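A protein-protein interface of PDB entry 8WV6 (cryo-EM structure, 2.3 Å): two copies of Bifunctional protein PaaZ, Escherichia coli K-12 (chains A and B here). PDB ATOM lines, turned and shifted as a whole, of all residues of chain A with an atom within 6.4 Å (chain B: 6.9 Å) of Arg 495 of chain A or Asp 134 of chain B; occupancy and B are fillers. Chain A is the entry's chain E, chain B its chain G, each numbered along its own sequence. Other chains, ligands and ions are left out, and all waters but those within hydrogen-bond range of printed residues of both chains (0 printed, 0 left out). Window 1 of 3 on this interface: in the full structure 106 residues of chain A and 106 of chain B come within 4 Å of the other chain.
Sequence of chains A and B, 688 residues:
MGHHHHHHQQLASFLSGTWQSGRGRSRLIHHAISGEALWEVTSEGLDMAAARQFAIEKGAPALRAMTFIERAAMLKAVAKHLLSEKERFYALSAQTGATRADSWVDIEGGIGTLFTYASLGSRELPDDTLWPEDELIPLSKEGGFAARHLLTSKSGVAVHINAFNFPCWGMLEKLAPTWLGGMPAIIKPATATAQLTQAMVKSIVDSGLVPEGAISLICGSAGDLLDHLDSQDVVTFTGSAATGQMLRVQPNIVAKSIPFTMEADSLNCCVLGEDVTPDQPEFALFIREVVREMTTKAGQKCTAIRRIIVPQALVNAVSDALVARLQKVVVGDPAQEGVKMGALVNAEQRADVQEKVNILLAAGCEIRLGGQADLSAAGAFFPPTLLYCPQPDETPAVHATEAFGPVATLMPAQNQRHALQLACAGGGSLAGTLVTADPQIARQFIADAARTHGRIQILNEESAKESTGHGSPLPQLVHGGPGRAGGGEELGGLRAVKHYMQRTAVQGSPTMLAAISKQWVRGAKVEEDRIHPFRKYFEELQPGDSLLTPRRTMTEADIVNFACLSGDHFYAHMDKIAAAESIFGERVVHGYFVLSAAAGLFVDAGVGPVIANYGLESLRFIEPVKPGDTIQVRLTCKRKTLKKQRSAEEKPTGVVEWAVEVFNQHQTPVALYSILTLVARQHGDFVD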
ATOM      1  N   TYR A 117      10.551 -12.608  10.332  1.00  0.00           N
ATOM      2  CA  TYR A 117      10.651 -11.515   9.376  1.00  0.00           C
ATOM      3  C   TYR A 117      12.104 -11.208   9.038  1.00  0.00           C
ATOM      4  O   TYR A 117      12.415 -10.891   7.887  1.00  0.00           O
ATOM      5  CB  TYR A 117       9.921 -10.286   9.902  1.00  0.00           C
ATOM      6  CG  TYR A 117       8.506 -10.234   9.385  1.00  0.00           C
ATOM      7  CD1 TYR A 117       8.223  -9.652   8.165  1.00  0.00           C
ATOM      8  CD2 TYR A 117       7.465 -10.806  10.093  1.00  0.00           C
ATOM      9  CE1 TYR A 117       6.946  -9.613   7.681  1.00  0.00           C
ATOM     10  CE2 TYR A 117       6.178 -10.776   9.609  1.00  0.00           C
ATOM     11  CZ  TYR A 117       5.929 -10.177   8.399  1.00  0.00           C
ATOM     12  OH  TYR A 117       4.658 -10.132   7.903  1.00  0.00           O
ATOM     13  N   TRP A 131      12.934  -1.407  -3.809  1.00  0.00           N
ATOM     14  CA  TRP A 131      12.513  -2.795  -4.016  1.00  0.00           C
ATOM     15  C   TRP A 131      11.801  -2.957  -5.355  1.00  0.00           C
ATOM     16  O   TRP A 131      10.604  -2.644  -5.464  1.00  0.00           O
ATOM     17  CB  TRP A 131      11.617  -3.247  -2.862  1.00  0.00           C
ATOM     18  CG  TRP A 131      11.135  -4.680  -2.927  1.00  0.00           C
ATOM     19  CD1 TRP A 131      11.493  -5.632  -3.835  1.00  0.00           C
ATOM     20  CD2 TRP A 131      10.202  -5.306  -2.042  1.00  0.00           C
ATOM     21  NE1 TRP A 131      10.845  -6.806  -3.571  1.00  0.00           N
ATOM     22  CE2 TRP A 131      10.044  -6.633  -2.475  1.00  0.00           C
ATOM     23  CE3 TRP A 131       9.486  -4.873  -0.924  1.00  0.00           C
ATOM     24  CZ2 TRP A 131       9.202  -7.528  -1.833  1.00  0.00           C
ATOM     25  CZ3 TRP A 131       8.655  -5.766  -0.286  1.00  0.00           C
ATOM     26  CH2 TRP A 131       8.517  -7.074  -0.739  1.00  0.00           C
ATOM     27  N   GLN A 476       3.708 -16.145   8.617  1.00  0.00           N
ATOM     28  CA  GLN A 476       3.713 -16.364   7.177  1.00  0.00           C
ATOM     29  C   GLN A 476       2.328 -16.239   6.549  1.00  0.00           C
ATOM     30  O   GLN A 476       2.225 -16.207   5.321  1.00  0.00           O
ATOM     31  CB  GLN A 476       4.298 -17.743   6.855  1.00  0.00           C
ATOM     32  CG  GLN A 476       5.727 -17.960   7.316  1.00  0.00           C
ATOM     33  CD  GLN A 476       5.820 -18.749   8.611  1.00  0.00           C
ATOM     34  OE1 GLN A 476       5.018 -18.573   9.526  1.00  0.00           O
ATOM     35  NE2 GLN A 476       6.805 -19.629   8.688  1.00  0.00           N
ATOM     36  N   LEU A 477       1.271 -16.159   7.349  1.00  0.00           N
ATOM     37  CA  LEU A 477      -0.101 -16.197   6.867  1.00  0.00           C
ATOM     38  C   LEU A 477      -0.814 -14.897   7.206  1.00  0.00           C
ATOM     39  O   LEU A 477      -0.572 -14.308   8.262  1.00  0.00           O
ATOM     40  CB  LEU A 477      -0.855 -17.370   7.486  1.00  0.00           C
ATOM     41  CG  LEU A 477      -0.175 -18.743   7.499  1.00  0.00           C
ATOM     42  CD1 LEU A 477      -1.132 -19.782   8.024  1.00  0.00           C
ATOM     43  CD2 LEU A 477       0.314 -19.131   6.123  1.00  0.00           C
ATOM     44  N   VAL A 478      -1.708 -14.462   6.316  1.00  0.00           N
ATOM     45  CA  VAL A 478      -2.435 -13.224   6.550  1.00  0.00           C
ATOM     46  C   VAL A 478      -3.248 -13.351   7.826  1.00  0.00           C
ATOM     47  O   VAL A 478      -3.631 -14.452   8.241  1.00  0.00           O
ATOM     48  CB  VAL A 478      -3.334 -12.873   5.352  1.00  0.00           C
ATOM     49  CG1 VAL A 478      -2.495 -12.544   4.125  1.00  0.00           C
ATOM     50  CG2 VAL A 478      -4.327 -13.997   5.071  1.00  0.00           C
ATOM     51  N   GLU A 489      -5.741  -6.497   6.954  1.00  0.00           N
ATOM     52  CA  GLU A 489      -4.868  -7.626   6.670  1.00  0.00           C
ATOM     53  C   GLU A 489      -3.513  -7.369   7.311  1.00  0.00           C
ATOM     54  O   GLU A 489      -2.948  -6.285   7.165  1.00  0.00           O
ATOM     55  CB  GLU A 489      -4.705  -7.845   5.160  1.00  0.00           C
ATOM     56  CG  GLU A 489      -4.451  -9.287   4.745  1.00  0.00           C
ATOM     57  CD  GLU A 489      -4.043  -9.427   3.278  1.00  0.00           C
ATOM     58  OE1 GLU A 489      -2.891  -9.078   2.941  1.00  0.00           O
ATOM     59  OE2 GLU A 489      -4.869  -9.890   2.460  1.00  0.00           O
ATOM     60  N   LEU A 491       0.394  -9.476   8.666  1.00  0.00           N
ATOM     61  CA  LEU A 491       1.249 -10.647   8.860  1.00  0.00           C
ATOM     62  C   LEU A 491       1.328 -11.578   7.659  1.00  0.00           C
ATOM     63  O   LEU A 491       1.582 -12.769   7.827  1.00  0.00           O
ATOM     64  CB  LEU A 491       0.786 -11.457  10.072  1.00  0.00           C
ATOM     65  CG  LEU A 491       1.238 -11.005  11.451  1.00  0.00           C
ATOM     66  CD1 LEU A 491       0.939 -12.101  12.445  1.00  0.00           C
ATOM     67  CD2 LEU A 491       2.703 -10.652  11.437  1.00  0.00           C
ATOM     68  N   GLY A 492       1.151 -11.109   6.438  1.00  0.00           N
ATOM     69  CA  GLY A 492       1.133 -12.072   5.352  1.00  0.00           C
ATOM     70  C   GLY A 492       2.480 -12.354   4.721  1.00  0.00           C
ATOM     71  O   GLY A 492       2.567 -12.523   3.505  1.00  0.00           O
ATOM     72  N   GLY A 493       3.531 -12.439   5.529  1.00  0.00           N
ATOM     73  CA  GLY A 493       4.872 -12.470   4.970  1.00  0.00           C
ATOM     74  C   GLY A 493       5.283 -11.078   4.521  1.00  0.00           C
ATOM     75  O   GLY A 493       5.016 -10.085   5.201  1.00  0.00           O
ATOM     76  N   LEU A 494       5.922 -10.998   3.351  1.00  0.00           N
ATOM     77  CA  LEU A 494       6.305  -9.709   2.780  1.00  0.00           C
ATOM     78  C   LEU A 494       5.096  -8.864   2.384  1.00  0.00           C
ATOM     79  O   LEU A 494       5.239  -7.652   2.134  1.00  0.00           O
ATOM     80  CB  LEU A 494       7.203  -9.928   1.565  1.00  0.00           C
ATOM     81  CG  LEU A 494       8.455 -10.782   1.767  1.00  0.00           C
ATOM     82  CD1 LEU A 494       9.205 -10.922   0.466  1.00  0.00           C
ATOM     83  CD2 LEU A 494       9.355 -10.210   2.840  1.00  0.00           C
ATOM     84  N   ARG A 495       3.918  -9.483   2.307  1.00  0.00           N
ATOM     85  CA  ARG A 495       2.695  -8.735   2.058  1.00  0.00           C
ATOM     86  C   ARG A 495       2.519  -7.617   3.073  1.00  0.00           C
ATOM     87  O   ARG A 495       2.086  -6.517   2.723  1.00  0.00           O
ATOM     88  CB  ARG A 495       1.490  -9.672   2.098  1.00  0.00           C
ATOM     89  CG  ARG A 495       1.339 -10.587   0.905  1.00  0.00           C
ATOM     90  CD  ARG A 495       0.059 -11.380   1.066  1.00  0.00           C
ATOM     91  NE  ARG A 495      -0.057 -12.518   0.166  1.00  0.00           N
ATOM     92  CZ  ARG A 495       0.528 -13.694   0.357  1.00  0.00           C
ATOM     93  NH1 ARG A 495       1.285 -13.908   1.418  1.00  0.00           N
ATOM     94  NH2 ARG A 495       0.351 -14.664  -0.519  1.00  0.00           N
ATOM     95  N   ALA A 496       2.884  -7.871   4.331  1.00  0.00           N
ATOM     96  CA  ALA A 496       2.746  -6.855   5.365  1.00  0.00           C
ATOM     97  C   ALA A 496       3.822  -5.782   5.242  1.00  0.00           C
ATOM     98  O   ALA A 496       3.579  -4.616   5.564  1.00  0.00           O
ATOM     99  CB  ALA A 496       2.785  -7.507   6.745  1.00  0.00           C
ATOM    100  N   VAL A 497       5.019  -6.154   4.782  1.00  0.00           N
ATOM    101  CA  VAL A 497       6.057  -5.159   4.527  1.00  0.00           C
ATOM    102  C   VAL A 497       5.581  -4.146   3.496  1.00  0.00           C
ATOM    103  O   VAL A 497       5.900  -2.956   3.580  1.00  0.00           O
ATOM    104  CB  VAL A 497       7.366  -5.836   4.074  1.00  0.00           C
ATOM    105  CG1 VAL A 497       8.452  -4.797   3.861  1.00  0.00           C
ATOM    106  CG2 VAL A 497       7.816  -6.871   5.075  1.00  0.00           C
ATOM    107  N   LYS A 498       4.824  -4.601   2.496  1.00  0.00           N
ATOM    108  CA  LYS A 498       4.387  -3.661   1.461  1.00  0.00           C
ATOM    109  C   LYS A 498       3.345  -2.642   1.929  1.00  0.00           C
ATOM    110  O   LYS A 498       3.001  -1.755   1.148  1.00  0.00           O
ATOM    111  CB  LYS A 498       3.830  -4.402   0.248  1.00  0.00           C
ATOM    112  CG  LYS A 498       4.861  -5.187  -0.515  1.00  0.00           C
ATOM    113  CD  LYS A 498       4.230  -6.102  -1.525  1.00  0.00           C
ATOM    114  CE  LYS A 498       5.078  -7.333  -1.727  1.00  0.00           C
ATOM    115  NZ  LYS A 498       5.386  -7.541  -3.154  1.00  0.00           N
ATOM    116  N   HIS A 499       2.825  -2.732   3.153  1.00  0.00           N
ATOM    117  CA  HIS A 499       1.846  -1.738   3.590  1.00  0.00           C
ATOM    118  C   HIS A 499       2.495  -0.435   4.022  1.00  0.00           C
ATOM    119  O   HIS A 499       1.807   0.579   4.133  1.00  0.00           O
ATOM    120  CB  HIS A 499       0.991  -2.264   4.742  1.00  0.00           C
ATOM    121  CG  HIS A 499       0.229  -3.504   4.410  1.00  0.00           C
ATOM    122  ND1 HIS A 499      -0.207  -3.790   3.135  1.00  0.00           N
ATOM    123  CD2 HIS A 499      -0.167  -4.540   5.185  1.00  0.00           C
ATOM    124  CE1 HIS A 499      -0.841  -4.948   3.140  1.00  0.00           C
ATOM    125  NE2 HIS A 499      -0.830  -5.424   4.371  1.00  0.00           N
ATOM    126  N   TRP B 131      -8.603 -19.532  -6.803  1.00  0.00           N
ATOM    127  CA  TRP B 131      -7.286 -19.112  -7.279  1.00  0.00           C
ATOM    128  C   TRP B 131      -6.232 -19.287  -6.190  1.00  0.00           C
ATOM    129  O   TRP B 131      -6.106 -18.428  -5.302  1.00  0.00           O
ATOM    130  CB  TRP B 131      -7.342 -17.662  -7.758  1.00  0.00           C
ATOM    131  CG  TRP B 131      -6.041 -17.096  -8.270  1.00  0.00           C
ATOM    132  CD1 TRP B 131      -4.866 -17.761  -8.462  1.00  0.00           C
ATOM    133  CD2 TRP B 131      -5.798 -15.742  -8.648  1.00  0.00           C
ATOM    134  NE1 TRP B 131      -3.911 -16.904  -8.933  1.00  0.00           N
ATOM    135  CE2 TRP B 131      -4.458 -15.656  -9.057  1.00  0.00           C
ATOM    136  CE3 TRP B 131      -6.587 -14.592  -8.683  1.00  0.00           C
ATOM    137  CZ2 TRP B 131      -3.890 -14.469  -9.492  1.00  0.00           C
ATOM    138  CZ3 TRP B 131      -6.023 -13.418  -9.121  1.00  0.00           C
ATOM    139  CH2 TRP B 131      -4.689 -13.362  -9.519  1.00  0.00           C
ATOM    140  N   PRO B 132      -5.456 -20.373  -6.214  1.00  0.00           N
ATOM    141  CA  PRO B 132      -4.317 -20.522  -5.292  1.00  0.00           C
ATOM    142  C   PRO B 132      -3.177 -19.615  -5.731  1.00  0.00           C
ATOM    143  O   PRO B 132      -2.619 -19.802  -6.813  1.00  0.00           O
ATOM    144  CB  PRO B 132      -3.941 -22.003  -5.432  1.00  0.00           C
ATOM    145  CG  PRO B 132      -5.068 -22.638  -6.165  1.00  0.00           C
ATOM    146  CD  PRO B 132      -5.651 -21.577  -7.030  1.00  0.00           C
ATOM    147  N   GLU B 133      -2.825 -18.634  -4.900  1.00  0.00           N
ATOM    148  CA  GLU B 133      -1.927 -17.589  -5.385  1.00  0.00           C
ATOM    149  C   GLU B 133      -0.446 -17.874  -5.148  1.00  0.00           C
ATOM    150  O   GLU B 133       0.373 -17.585  -6.023  1.00  0.00           O
ATOM    151  CB  GLU B 133      -2.304 -16.233  -4.783  1.00  0.00           C
ATOM    152  CG  GLU B 133      -2.004 -16.043  -3.324  1.00  0.00           C
ATOM    153  CD  GLU B 133      -2.042 -14.584  -2.912  1.00  0.00           C
ATOM    154  OE1 GLU B 133      -2.170 -13.717  -3.795  1.00  0.00           O
ATOM    155  OE2 GLU B 133      -1.953 -14.305  -1.702  1.00  0.00           O
ATOM    156  N   ASP B 134      -0.063 -18.423  -4.003  1.00  0.00           N
ATOM    157  CA  ASP B 134       1.338 -18.716  -3.737  1.00  0.00           C
ATOM    158  C   ASP B 134       1.566 -20.222  -3.718  1.00  0.00           C
ATOM    159  O   ASP B 134       0.629 -21.011  -3.819  1.00  0.00           O
ATOM    160  CB  ASP B 134       1.800 -18.080  -2.416  1.00  0.00           C
ATOM    161  CG  ASP B 134       0.924 -18.462  -1.219  1.00  0.00           C
ATOM    162  OD1 ASP B 134       0.583 -17.564  -0.424  1.00  0.00           O
ATOM    163  OD2 ASP B 134       0.594 -19.651  -1.044  1.00  0.00           O
ATOM    164  N   GLU B 135       2.827 -20.615  -3.563  1.00  0.00           N
ATOM    165  CA  GLU B 135       3.172 -22.021  -3.414  1.00  0.00           C
ATOM    166  C   GLU B 135       2.882 -22.500  -1.994  1.00  0.00           C
ATOM    167  O   GLU B 135       2.553 -21.722  -1.103  1.00  0.00           O
ATOM    168  CB  GLU B 135       4.640 -22.260  -3.756  1.00  0.00           C
ATOM    169  CG  GLU B 135       4.984 -22.034  -5.219  1.00  0.00           C
ATOM    170  CD  GLU B 135       4.108 -22.840  -6.162  1.00  0.00           C
ATOM    171  OE1 GLU B 135       4.180 -24.083  -6.134  1.00  0.00           O
ATOM    172  OE2 GLU B 135       3.342 -22.229  -6.936  1.00  0.00           O
ATOM    173  N   LEU B 136       3.005 -23.807  -1.789  1.00  0.00           N
ATOM    174  CA  LEU B 136       2.717 -24.383  -0.483  1.00  0.00           C
ATOM    175  C   LEU B 136       3.768 -23.975   0.539  1.00  0.00           C
ATOM    176  O   LEU B 136       4.969 -24.057   0.287  1.00  0.00           O
ATOM    177  CB  LEU B 136       2.649 -25.903  -0.578  1.00  0.00           C
ATOM    178  CG  LEU B 136       2.324 -26.620   0.730  1.00  0.00           C
ATOM    179  CD1 LEU B 136       0.840 -26.751   0.872  1.00  0.00           C
ATOM    180  CD2 LEU B 136       2.991 -27.970   0.790  1.00  0.00           C
ATOM    181  N   ILE B 137       3.303 -23.532   1.700  1.00  0.00           N
ATOM    182  CA  ILE B 137       4.128 -23.078   2.814  1.00  0.00           C
ATOM    183  C   ILE B 137       4.219 -24.222   3.820  1.00  0.00           C
ATOM    184  O   ILE B 137       3.202 -24.596   4.418  1.00  0.00           O
ATOM    185  CB  ILE B 137       3.541 -21.819   3.469  1.00  0.00           C
ATOM    186  CG1 ILE B 137       3.357 -20.707   2.442  1.00  0.00           C
ATOM    187  CG2 ILE B 137       4.410 -21.348   4.618  1.00  0.00           C
ATOM    188  CD1 ILE B 137       2.467 -19.588   2.926  1.00  0.00           C
ATOM    189  N   ALA B 147       0.266 -24.858   4.690  1.00  0.00           N
ATOM    190  CA  ALA B 147      -0.677 -23.793   4.384  1.00  0.00           C
ATOM    191  C   ALA B 147      -0.391 -23.244   2.995  1.00  0.00           C
ATOM    192  O   ALA B 147       0.724 -23.360   2.484  1.00  0.00           O
ATOM    193  CB  ALA B 147      -0.616 -22.674   5.431  1.00  0.00           C
ATOM    194  N   ARG B 148      -1.421 -22.666   2.381  1.00  0.00           N
ATOM    195  CA  ARG B 148      -1.244 -21.805   1.217  1.00  0.00           C
ATOM    196  C   ARG B 148      -2.400 -20.818   1.171  1.00  0.00           C
ATOM    197  O   ARG B 148      -3.413 -20.999   1.842  1.00  0.00           O
ATOM    198  CB  ARG B 148      -1.135 -22.601  -0.091  1.00  0.00           C
ATOM    199  CG  ARG B 148      -2.372 -23.328  -0.534  1.00  0.00           C
ATOM    200  CD  ARG B 148      -2.063 -24.314  -1.668  1.00  0.00           C
ATOM    201  NE  ARG B 148      -1.332 -23.714  -2.781  1.00  0.00           N
ATOM    202  CZ  ARG B 148      -1.306 -24.210  -4.016  1.00  0.00           C
ATOM    203  NH1 ARG B 148      -1.969 -25.314  -4.310  1.00  0.00           N
ATOM    204  NH2 ARG B 148      -0.614 -23.599  -4.960  1.00  0.00           N
ATOM    205  N   HIS B 149      -2.224 -19.750   0.399  1.00  0.00           N
ATOM    206  CA  HIS B 149      -3.227 -18.698   0.302  1.00  0.00           C
ATOM    207  C   HIS B 149      -4.109 -18.919  -0.918  1.00  0.00           C
ATOM    208  O   HIS B 149      -3.619 -19.281  -1.988  1.00  0.00           O
ATOM    209  CB  HIS B 149      -2.578 -17.319   0.229  1.00  0.00           C
ATOM    210  CG  HIS B 149      -1.970 -16.867   1.517  1.00  0.00           C
ATOM    211  ND1 HIS B 149      -0.637 -17.041   1.803  1.00  0.00           N
ATOM    212  CD2 HIS B 149      -2.508 -16.254   2.595  1.00  0.00           C
ATOM    213  CE1 HIS B 149      -0.375 -16.546   2.997  1.00  0.00           C
ATOM    214  NE2 HIS B 149      -1.494 -16.061   3.500  1.00  0.00           N
ATOM    215  N   LEU B 150      -5.408 -18.707  -0.749  1.00  0.00           N
ATOM    216  CA  LEU B 150      -6.373 -18.810  -1.829  1.00  0.00           C
ATOM    217  C   LEU B 150      -7.134 -17.504  -1.974  1.00  0.00           C
ATOM    218  O   LEU B 150      -7.314 -16.761  -1.011  1.00  0.00           O
ATOM    219  CB  LEU B 150      -7.386 -19.927  -1.597  1.00  0.00           C
ATOM    220  CG  LEU B 150      -6.914 -21.304  -1.164  1.00  0.00           C
ATOM    221  CD1 LEU B 150      -8.131 -22.171  -0.994  1.00  0.00           C
ATOM    222  CD2 LEU B 150      -5.993 -21.912  -2.185  1.00  0.00           C
ATOM    223  N   ARG B 503      -8.761 -12.859   0.183  1.00  0.00           N
ATOM    224  CA  ARG B 503      -7.581 -13.693   0.364  1.00  0.00           C
ATOM    225  C   ARG B 503      -7.708 -14.462   1.669  1.00  0.00           C
ATOM    226  O   ARG B 503      -8.008 -13.876   2.712  1.00  0.00           O
ATOM    227  CB  ARG B 503      -6.310 -12.847   0.367  1.00  0.00           C
ATOM    228  CG  ARG B 503      -5.029 -13.625   0.620  1.00  0.00           C
ATOM    229  CD  ARG B 503      -3.809 -12.713   0.706  1.00  0.00           C
ATOM    230  NE  ARG B 503      -3.405 -12.163  -0.586  1.00  0.00           N
ATOM    231  CZ  ARG B 503      -3.777 -10.973  -1.049  1.00  0.00           C
ATOM    232  NH1 ARG B 503      -4.569 -10.192  -0.338  1.00  0.00           N
ATOM    233  NH2 ARG B 503      -3.362 -10.566  -2.235  1.00  0.00           N
ATOM    234  N   GLN B 519      -4.996 -28.689  -7.263  1.00  0.00           N
ATOM    235  CA  GLN B 519      -3.635 -28.847  -7.741  1.00  0.00           C
ATOM    236  C   GLN B 519      -2.890 -29.707  -6.738  1.00  0.00           C
ATOM    237  O   GLN B 519      -3.076 -29.571  -5.530  1.00  0.00           O
ATOM    238  CB  GLN B 519      -2.900 -27.508  -7.900  1.00  0.00           C
ATOM    239  CG  GLN B 519      -3.657 -26.446  -8.664  1.00  0.00           C
ATOM    240  CD  GLN B 519      -2.984 -25.097  -8.608  1.00  0.00           C
ATOM    241  OE1 GLN B 519      -1.995 -24.915  -7.910  1.00  0.00           O
ATOM    242  NE2 GLN B 519      -3.522 -24.139  -9.344  1.00  0.00           N
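The backbone NH (N) of Val 478 of chain A sits at hydrogen-bond distance from a ring nitrogen (NE2) of His 149 of chain B (3.2 Å).
OE2 of Glu 489 of chain A lies within salt-bridge range of NH1 of Arg 503 of chain B, at 2.8 Å.
The side-chain carboxylate of Glu 133 of chain B is in salt-bridge range of the guanidinium group of Arg 495 of chain A.
The side-chain carboxylate of Asp 134 of chain B is in salt-bridge range of the guanidinium group of Arg 495 of chain A, at 2.9 Å.
ND1 of His 149 of chain B is in hydrogen-bond range of NH2 of Arg 495 of chain A.
The guanidinium group (NE) of Arg 495 of chain A lies close to the guanidinium group (NE) of Arg 503 of chain B (3.4 Å).
The backbone NH of Leu 477 of chain A lies close to the backbone carbonyl oxygen of Leu 491 of chain A (3.4 Å).
The backbone carbonyl oxygen of Gly 492 of chain A sits at hydrogen-bond distance from the guanidinium group of Arg 495 of chain A.
OE2 of Glu 133 of chain B lies within salt-bridge range of NE of Arg 503 of chain B, at 2.8 Å.
NH2 of Arg 148 of chain B is in hydrogen-bond range of O of Asp 134 of chain B (3.1 Å).
ND1 of His 149 of chain B lies within hydrogen-bond range of OD1 of Asp 134 of chain B, at 2.6 Å.
N of Ile 137 of chain B sits at hydrogen-bond distance from O of Ala 147 of chain B (2.7 Å).
His 149 of chain B touches Gln 476 of chain A (CE1 to O, 3.5 Å).
CD2 of Leu 477 of chain A touches CD1 of Ile 137 of chain B, at 3.9 Å.
Ala 147 of chain B touches Leu 477 of chain A (CB to CD2, 3.7 Å).
Leu 477 of chain A touches His 149 of chain B (CA to NE2, 3.6 Å).
CD of Arg 503 of chain B touches CG1 of Val 478 of chain A (3.7 Å).
Of chain B, only Glu 133 (2.6 Å), Asp 134 (2.9 Å), His 149 (3.5 Å) and Arg 503 (3.4 Å) come within 4 Å of Arg 495 of chain A.
Of chain A, only Arg 495 comes within 4 Å of Asp 134 of chain B.
Printed residues of chain A within 4 Å of Ala 147 of chain B: Leu 477 (3.7 Å).
Of the printed residues of chain A, His 149 of chain B touches Gln 476, Leu 477, Val 478 and Arg 495.
Printed residues of chain B within 4 Å of Gln 476 of chain A: His 149.
Printed residues of chain A within 4 Å of Glu 133 of chain B: Arg 495.
Of the printed residues of chain B, Glu 489 of chain A touches Arg 503.
Pro 132 of chain B touches none of the printed residues of chain A.
Trp 131 of chain A touches none of the printed residues of chain B.
The nearest residue of chain A that does not touch Asp 134 of chain B is Gln 476 of chain A (6.1 Å).
Printed residues of chain A that touch a printed residue of chain B: Gln 476, Leu 477, Val 478, Glu 489 and Arg 495.
Hydrophobic or aromatic side chains of chain A that line the printed part of chain B: Leu 477 and Val 478.
Printed residues of chain B that touch a printed residue of chain A: Glu 133, Asp 134, Ile 137, Ala 147, His 149 and Arg 503.
Hydrophobic or aromatic side chains of chain B that line the printed part of chain A: Ile 137, Ala 147 and His 149.
Position printed for both chains: 131.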
